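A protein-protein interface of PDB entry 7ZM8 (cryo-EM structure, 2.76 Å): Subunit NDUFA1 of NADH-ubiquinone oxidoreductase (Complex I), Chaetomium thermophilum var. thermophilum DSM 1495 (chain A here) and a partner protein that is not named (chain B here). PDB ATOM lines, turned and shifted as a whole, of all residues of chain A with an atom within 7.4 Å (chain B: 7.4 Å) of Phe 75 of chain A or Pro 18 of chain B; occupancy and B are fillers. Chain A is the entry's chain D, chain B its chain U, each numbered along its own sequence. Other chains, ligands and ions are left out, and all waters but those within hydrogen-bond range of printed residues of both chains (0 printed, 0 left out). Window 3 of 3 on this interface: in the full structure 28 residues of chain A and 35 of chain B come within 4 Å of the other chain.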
ATOM      1  N   ARG A  55     -13.622   2.140  26.431  1.00  0.00           N
ATOM      2  CA  ARG A  55     -13.961   3.441  27.057  1.00  0.00           C
ATOM      3  C   ARG A  55     -13.890   3.316  28.582  1.00  0.00           C
ATOM      4  O   ARG A  55     -13.358   4.247  29.208  1.00  0.00           O
ATOM      5  CB  ARG A  55     -15.333   3.922  26.585  1.00  0.00           C
ATOM      6  CG  ARG A  55     -15.362   4.504  25.182  1.00  0.00           C
ATOM      7  CD  ARG A  55     -16.780   4.956  24.913  1.00  0.00           C
ATOM      8  NE  ARG A  55     -17.144   6.064  25.780  1.00  0.00           N
ATOM      9  CZ  ARG A  55     -18.383   6.493  25.969  1.00  0.00           C
ATOM     10  NH1 ARG A  55     -19.389   5.884  25.370  1.00  0.00           N
ATOM     11  NH2 ARG A  55     -18.620   7.517  26.767  1.00  0.00           N
ATOM     12  N   PRO A  70     -16.448   5.986  35.601  1.00  0.00           N
ATOM     13  CA  PRO A  70     -15.413   6.867  36.143  1.00  0.00           C
ATOM     14  C   PRO A  70     -15.523   8.263  35.563  1.00  0.00           C
ATOM     15  O   PRO A  70     -16.105   8.452  34.485  1.00  0.00           O
ATOM     16  CB  PRO A  70     -14.110   6.185  35.707  1.00  0.00           C
ATOM     17  CG  PRO A  70     -14.488   5.401  34.510  1.00  0.00           C
ATOM     18  CD  PRO A  70     -15.881   4.928  34.751  1.00  0.00           C
ATOM     19  N   PRO A  71     -14.992   9.274  36.253  1.00  0.00           N
ATOM     20  CA  PRO A  71     -15.024  10.634  35.701  1.00  0.00           C
ATOM     21  C   PRO A  71     -14.212  10.721  34.420  1.00  0.00           C
ATOM     22  O   PRO A  71     -13.178  10.070  34.272  1.00  0.00           O
ATOM     23  CB  PRO A  71     -14.423  11.498  36.817  1.00  0.00           C
ATOM     24  CG  PRO A  71     -14.179  10.590  37.976  1.00  0.00           C
ATOM     25  CD  PRO A  71     -14.205   9.189  37.492  1.00  0.00           C
ATOM     26  N   GLY A  72     -14.692  11.542  33.491  1.00  0.00           N
ATOM     27  CA  GLY A  72     -14.122  11.624  32.167  1.00  0.00           C
ATOM     28  C   GLY A  72     -14.681  10.629  31.175  1.00  0.00           C
ATOM     29  O   GLY A  72     -14.356  10.716  29.987  1.00  0.00           O
ATOM     30  N   PHE A  73     -15.510   9.686  31.626  1.00  0.00           N
ATOM     31  CA  PHE A  73     -16.112   8.724  30.713  1.00  0.00           C
ATOM     32  C   PHE A  73     -17.073   9.398  29.740  1.00  0.00           C
ATOM     33  O   PHE A  73     -17.255   8.917  28.617  1.00  0.00           O
ATOM     34  CB  PHE A  73     -16.829   7.630  31.504  1.00  0.00           C
ATOM     35  CG  PHE A  73     -17.568   6.652  30.644  1.00  0.00           C
ATOM     36  CD1 PHE A  73     -16.885   5.676  29.941  1.00  0.00           C
ATOM     37  CD2 PHE A  73     -18.941   6.718  30.526  1.00  0.00           C
ATOM     38  CE1 PHE A  73     -17.558   4.789  29.139  1.00  0.00           C
ATOM     39  CE2 PHE A  73     -19.618   5.828  29.729  1.00  0.00           C
ATOM     40  CZ  PHE A  73     -18.927   4.863  29.033  1.00  0.00           C
ATOM     41  N   GLU A  74     -17.691  10.505  30.141  1.00  0.00           N
ATOM     42  CA  GLU A  74     -18.603  11.212  29.255  1.00  0.00           C
ATOM     43  C   GLU A  74     -17.888  11.997  28.163  1.00  0.00           C
ATOM     44  O   GLU A  74     -18.554  12.695  27.394  1.00  0.00           O
ATOM     45  CB  GLU A  74     -19.495  12.149  30.066  1.00  0.00           C
ATOM     46  CG  GLU A  74     -18.793  13.385  30.594  1.00  0.00           C
ATOM     47  CD  GLU A  74     -18.171  13.158  31.949  1.00  0.00           C
ATOM     48  OE1 GLU A  74     -17.996  11.984  32.335  1.00  0.00           O
ATOM     49  OE2 GLU A  74     -17.864  14.154  32.633  1.00  0.00           O
ATOM     50  N   PHE A  75     -16.561  11.895  28.066  1.00  0.00           N
ATOM     51  CA  PHE A  75     -15.789  12.607  27.059  1.00  0.00           C
ATOM     52  C   PHE A  75     -15.005  11.712  26.112  1.00  0.00           C
ATOM     53  O   PHE A  75     -14.659  12.166  25.018  1.00  0.00           O
ATOM     54  CB  PHE A  75     -14.793  13.570  27.724  1.00  0.00           C
ATOM     55  CG  PHE A  75     -15.436  14.604  28.595  1.00  0.00           C
ATOM     56  CD1 PHE A  75     -16.191  15.618  28.045  1.00  0.00           C
ATOM     57  CD2 PHE A  75     -15.280  14.562  29.963  1.00  0.00           C
ATOM     58  CE1 PHE A  75     -16.779  16.564  28.844  1.00  0.00           C
ATOM     59  CE2 PHE A  75     -15.863  15.508  30.762  1.00  0.00           C
ATOM     60  CZ  PHE A  75     -16.615  16.508  30.202  1.00  0.00           C
ATOM     61  N   ASN A  76     -14.726  10.470  26.522  1.00  0.00           N
ATOM     62  CA  ASN A  76     -13.862   9.546  25.736  1.00  0.00           C
ATOM     63  C   ASN A  76     -14.644   8.765  24.673  1.00  0.00           C
ATOM     64  O   ASN A  76     -14.075   7.807  24.133  1.00  0.00           O
ATOM     65  CB  ASN A  76     -13.084   8.597  26.651  1.00  0.00           C
ATOM     66  CG  ASN A  76     -13.947   7.758  27.569  1.00  0.00           C
ATOM     67  OD1 ASN A  76     -15.142   7.602  27.346  1.00  0.00           O
ATOM     68  ND2 ASN A  76     -13.343   7.196  28.600  1.00  0.00           N
ATOM     69  N   ASN A  77     -15.879   9.164  24.373  1.00  0.00           N
ATOM     70  CA  ASN A  77     -16.658   8.474  23.357  1.00  0.00           C
ATOM     71  C   ASN A  77     -16.036   8.721  21.991  1.00  0.00           C
ATOM     72  O   ASN A  77     -15.949   9.878  21.562  1.00  0.00           O
ATOM     73  CB  ASN A  77     -18.099   8.964  23.393  1.00  0.00           C
ATOM     74  CG  ASN A  77     -19.041   8.058  22.641  1.00  0.00           C
ATOM     75  OD1 ASN A  77     -18.767   6.879  22.445  1.00  0.00           O
ATOM     76  ND2 ASN A  77     -20.169   8.609  22.213  1.00  0.00           N
ATOM     77  N   PRO A  78     -15.532   7.690  21.272  1.00  0.00           N
ATOM     78  CA  PRO A  78     -14.781   7.939  20.054  1.00  0.00           C
ATOM     79  C   PRO A  78     -15.664   8.256  18.855  1.00  0.00           C
ATOM     80  O   PRO A  78     -16.554   7.496  18.562  1.00  0.00           O
ATOM     81  CB  PRO A  78     -13.990   6.647  19.812  1.00  0.00           C
ATOM     82  CG  PRO A  78     -14.327   5.733  20.968  1.00  0.00           C
ATOM     83  CD  PRO A  78     -15.646   6.237  21.502  1.00  0.00           C
ATOM     84  N   LEU B  13     -11.906  11.830  16.848  1.00  0.00           N
ATOM     85  CA  LEU B  13     -12.068  13.232  17.310  1.00  0.00           C
ATOM     86  C   LEU B  13     -12.819  13.242  18.638  1.00  0.00           C
ATOM     87  O   LEU B  13     -13.974  12.803  18.658  1.00  0.00           O
ATOM     88  CB  LEU B  13     -12.794  14.061  16.249  1.00  0.00           C
ATOM     89  CG  LEU B  13     -12.933  15.550  16.554  1.00  0.00           C
ATOM     90  CD1 LEU B  13     -11.573  16.200  16.727  1.00  0.00           C
ATOM     91  CD2 LEU B  13     -13.720  16.248  15.459  1.00  0.00           C
ATOM     92  N   LEU B  14     -12.163  13.698  19.703  1.00  0.00           N
ATOM     93  CA  LEU B  14     -12.829  13.825  21.016  1.00  0.00           C
ATOM     94  C   LEU B  14     -13.196  15.287  21.231  1.00  0.00           C
ATOM     95  O   LEU B  14     -12.669  16.141  20.503  1.00  0.00           O
ATOM     96  CB  LEU B  14     -11.902  13.324  22.125  1.00  0.00           C
ATOM     97  CG  LEU B  14     -11.593  11.828  22.109  1.00  0.00           C
ATOM     98  CD1 LEU B  14     -10.734  11.445  23.301  1.00  0.00           C
ATOM     99  CD2 LEU B  14     -12.873  11.013  22.103  1.00  0.00           C
ATOM    100  N   ASP B  15     -14.089  15.549  22.176  1.00  0.00           N
ATOM    101  CA  ASP B  15     -14.546  16.892  22.503  1.00  0.00           C
ATOM    102  C   ASP B  15     -14.668  16.995  24.014  1.00  0.00           C
ATOM    103  O   ASP B  15     -15.549  16.366  24.608  1.00  0.00           O
ATOM    104  CB  ASP B  15     -15.885  17.189  21.824  1.00  0.00           C
ATOM    105  CG  ASP B  15     -16.125  18.669  21.617  1.00  0.00           C
ATOM    106  OD1 ASP B  15     -15.262  19.484  22.000  1.00  0.00           O
ATOM    107  OD2 ASP B  15     -17.184  19.017  21.061  1.00  0.00           O
ATOM    108  N   THR B  16     -13.785  17.776  24.634  1.00  0.00           N
ATOM    109  CA  THR B  16     -13.792  17.895  26.085  1.00  0.00           C
ATOM    110  C   THR B  16     -14.833  18.878  26.599  1.00  0.00           C
ATOM    111  O   THR B  16     -14.972  19.020  27.817  1.00  0.00           O
ATOM    112  CB  THR B  16     -12.417  18.311  26.598  1.00  0.00           C
ATOM    113  OG1 THR B  16     -12.251  19.722  26.434  1.00  0.00           O
ATOM    114  CG2 THR B  16     -11.334  17.594  25.833  1.00  0.00           C
ATOM    115  N   THR B  17     -15.553  19.551  25.718  1.00  0.00           N
ATOM    116  CA  THR B  17     -16.579  20.488  26.136  1.00  0.00           C
ATOM    117  C   THR B  17     -17.681  19.746  26.879  1.00  0.00           C
ATOM    118  O   THR B  17     -18.202  18.750  26.357  1.00  0.00           O
ATOM    119  CB  THR B  17     -17.161  21.212  24.930  1.00  0.00           C
ATOM    120  OG1 THR B  17     -16.098  21.760  24.143  1.00  0.00           O
ATOM    121  CG2 THR B  17     -18.081  22.332  25.380  1.00  0.00           C
ATOM    122  N   PRO B  18     -18.059  20.179  28.073  1.00  0.00           N
ATOM    123  CA  PRO B  18     -19.101  19.491  28.835  1.00  0.00           C
ATOM    124  C   PRO B  18     -20.486  19.945  28.395  1.00  0.00           C
ATOM    125  O   PRO B  18     -20.643  20.817  27.545  1.00  0.00           O
ATOM    126  CB  PRO B  18     -18.815  19.911  30.279  1.00  0.00           C
ATOM    127  CG  PRO B  18     -17.564  20.742  30.234  1.00  0.00           C
ATOM    128  CD  PRO B  18     -17.446  21.256  28.854  1.00  0.00           C
ATOM    129  N   LEU B  19     -21.512  19.326  28.990  1.00  0.00           N
ATOM    130  CA  LEU B  19     -22.909  19.734  28.700  1.00  0.00           C
ATOM    131  C   LEU B  19     -23.136  21.089  29.371  1.00  0.00           C
ATOM    132  O   LEU B  19     -22.425  21.382  30.348  1.00  0.00           O
ATOM    133  CB  LEU B  19     -23.865  18.683  29.271  1.00  0.00           C
ATOM    134  CG  LEU B  19     -24.219  17.516  28.353  1.00  0.00           C
ATOM    135  CD1 LEU B  19     -24.965  16.439  29.123  1.00  0.00           C
ATOM    136  CD2 LEU B  19     -25.051  17.990  27.174  1.00  0.00           C
ATOM    137  N   PRO B  20     -24.083  21.929  28.907  1.00  0.00           N
ATOM    138  CA  PRO B  20     -24.355  23.191  29.570  1.00  0.00           C
ATOM    139  C   PRO B  20     -24.960  22.964  30.961  1.00  0.00           C
ATOM    140  O   PRO B  20     -25.586  21.940  31.164  1.00  0.00           O
ATOM    141  CB  PRO B  20     -25.344  23.901  28.643  1.00  0.00           C
ATOM    142  CG  PRO B  20     -25.196  23.187  27.322  1.00  0.00           C
ATOM    143  CD  PRO B  20     -24.876  21.756  27.694  1.00  0.00           C
ATOM    144  N   ASP B  21     -24.774  23.918  31.879  1.00  0.00           N
ATOM    145  CA  ASP B  21     -25.249  23.758  33.280  1.00  0.00           C
ATOM    146  C   ASP B  21     -26.771  23.592  33.303  1.00  0.00           C
ATOM    147  O   ASP B  21     -27.267  22.901  34.212  1.00  0.00           O
ATOM    148  CB  ASP B  21     -24.813  24.946  34.140  1.00  0.00           C
ATOM    149  CG  ASP B  21     -24.880  24.676  35.633  1.00  0.00           C
ATOM    150  OD1 ASP B  21     -24.847  23.491  36.016  1.00  0.00           O
ATOM    151  OD2 ASP B  21     -24.967  25.655  36.401  1.00  0.00           O
ATOM    152  N   LYS B  25     -27.784  17.136  35.427  1.00  0.00           N
ATOM    153  CA  LYS B  25     -26.708  16.143  35.145  1.00  0.00           C
ATOM    154  C   LYS B  25     -27.098  14.717  35.551  1.00  0.00           C
ATOM    155  O   LYS B  25     -28.066  14.563  36.317  1.00  0.00           O
ATOM    156  CB  LYS B  25     -25.399  16.581  35.810  1.00  0.00           C
ATOM    157  CG  LYS B  25     -24.828  17.891  35.288  1.00  0.00           C
ATOM    158  CD  LYS B  25     -23.565  18.329  35.995  1.00  0.00           C
ATOM    159  CE  LYS B  25     -23.001  19.619  35.442  1.00  0.00           C
ATOM    160  NZ  LYS B  25     -23.998  20.716  35.488  1.00  0.00           N
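Pro 71 of chain A touches none of the printed residues of chain B.
Of the printed residues of chain B, Phe 75 of chain A touches Leu 14, Asp 15, Thr 16, Thr 17 and Pro 18.
Of the printed residues of chain B, Asn 76 of chain A touches Leu 14.
Printed residues of chain A within 4 Å of Leu 14 of chain B: Phe 75 (3.6 Å), Asn 76 (3.8 Å) and Asn 77 (3.3 Å).
Printed residues of chain A within 4 Å of Asp 15 of chain B: Phe 75 (3.6 Å).
Of the printed residues of chain A, Thr 16 of chain B touches Phe 75.
Of the printed residues of chain A, Thr 17 of chain B touches Phe 75.
Pro 18 of chain B touches just one residue of chain A: Phe 75 (3.7 Å).
Asp 21 of chain B touches none of the printed residues of chain A.
The nearest residue of chain B that does not touch Phe 75 of chain A is Leu 19 of chain B (5.5 Å).
The nearest printed residue of chain A that does not touch Thr 16 of chain B is Glu 74 of chain A (7.2 Å).
Among the printed residues, merely in contact across the chains: Phe 75 of chain A with Leu 14 of chain B, Phe 75 of chain A with Asp 15 of chain B, Phe 75 of chain A with Thr 16 of chain B, Phe 75 of chain A with Thr 17 of chain B, Phe 75 of chain A with Pro 18 of chain B, Asn 76 of chain A with Leu 14 of chain B and Asn 77 of chain A with Leu 14 of chain B.
The side-chain carboxylate (OD1) of Asp 15 of chain B sits at hydrogen-bond distance from the side-chain hydroxyl (OG1) of Thr 17 of chain B (3.2 Å).
The side-chain amide oxygen (OD1) of Asn 76 of chain A lies within hydrogen-bond range of the guanidinium group (NE) of Arg 55 of chain A.
OD1 of Asn 77 of chain A is in hydrogen-bond range of NH1 of Arg 55 of chain A (3.2 Å).
The backbone carbonyl oxygen of Phe 73 of chain A sits close to the side-chain amide oxygen of Asn 76 of chain A.
Hydrophobic or aromatic side chains of chain B within 4 Å of the printed part of chain A: Leu 14.
Of the 10 printed residues of chain A, 3 touch a printed residue of chain B.
Along chain A the printed residues that touch a printed residue of chain B span positions 75 to 77.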
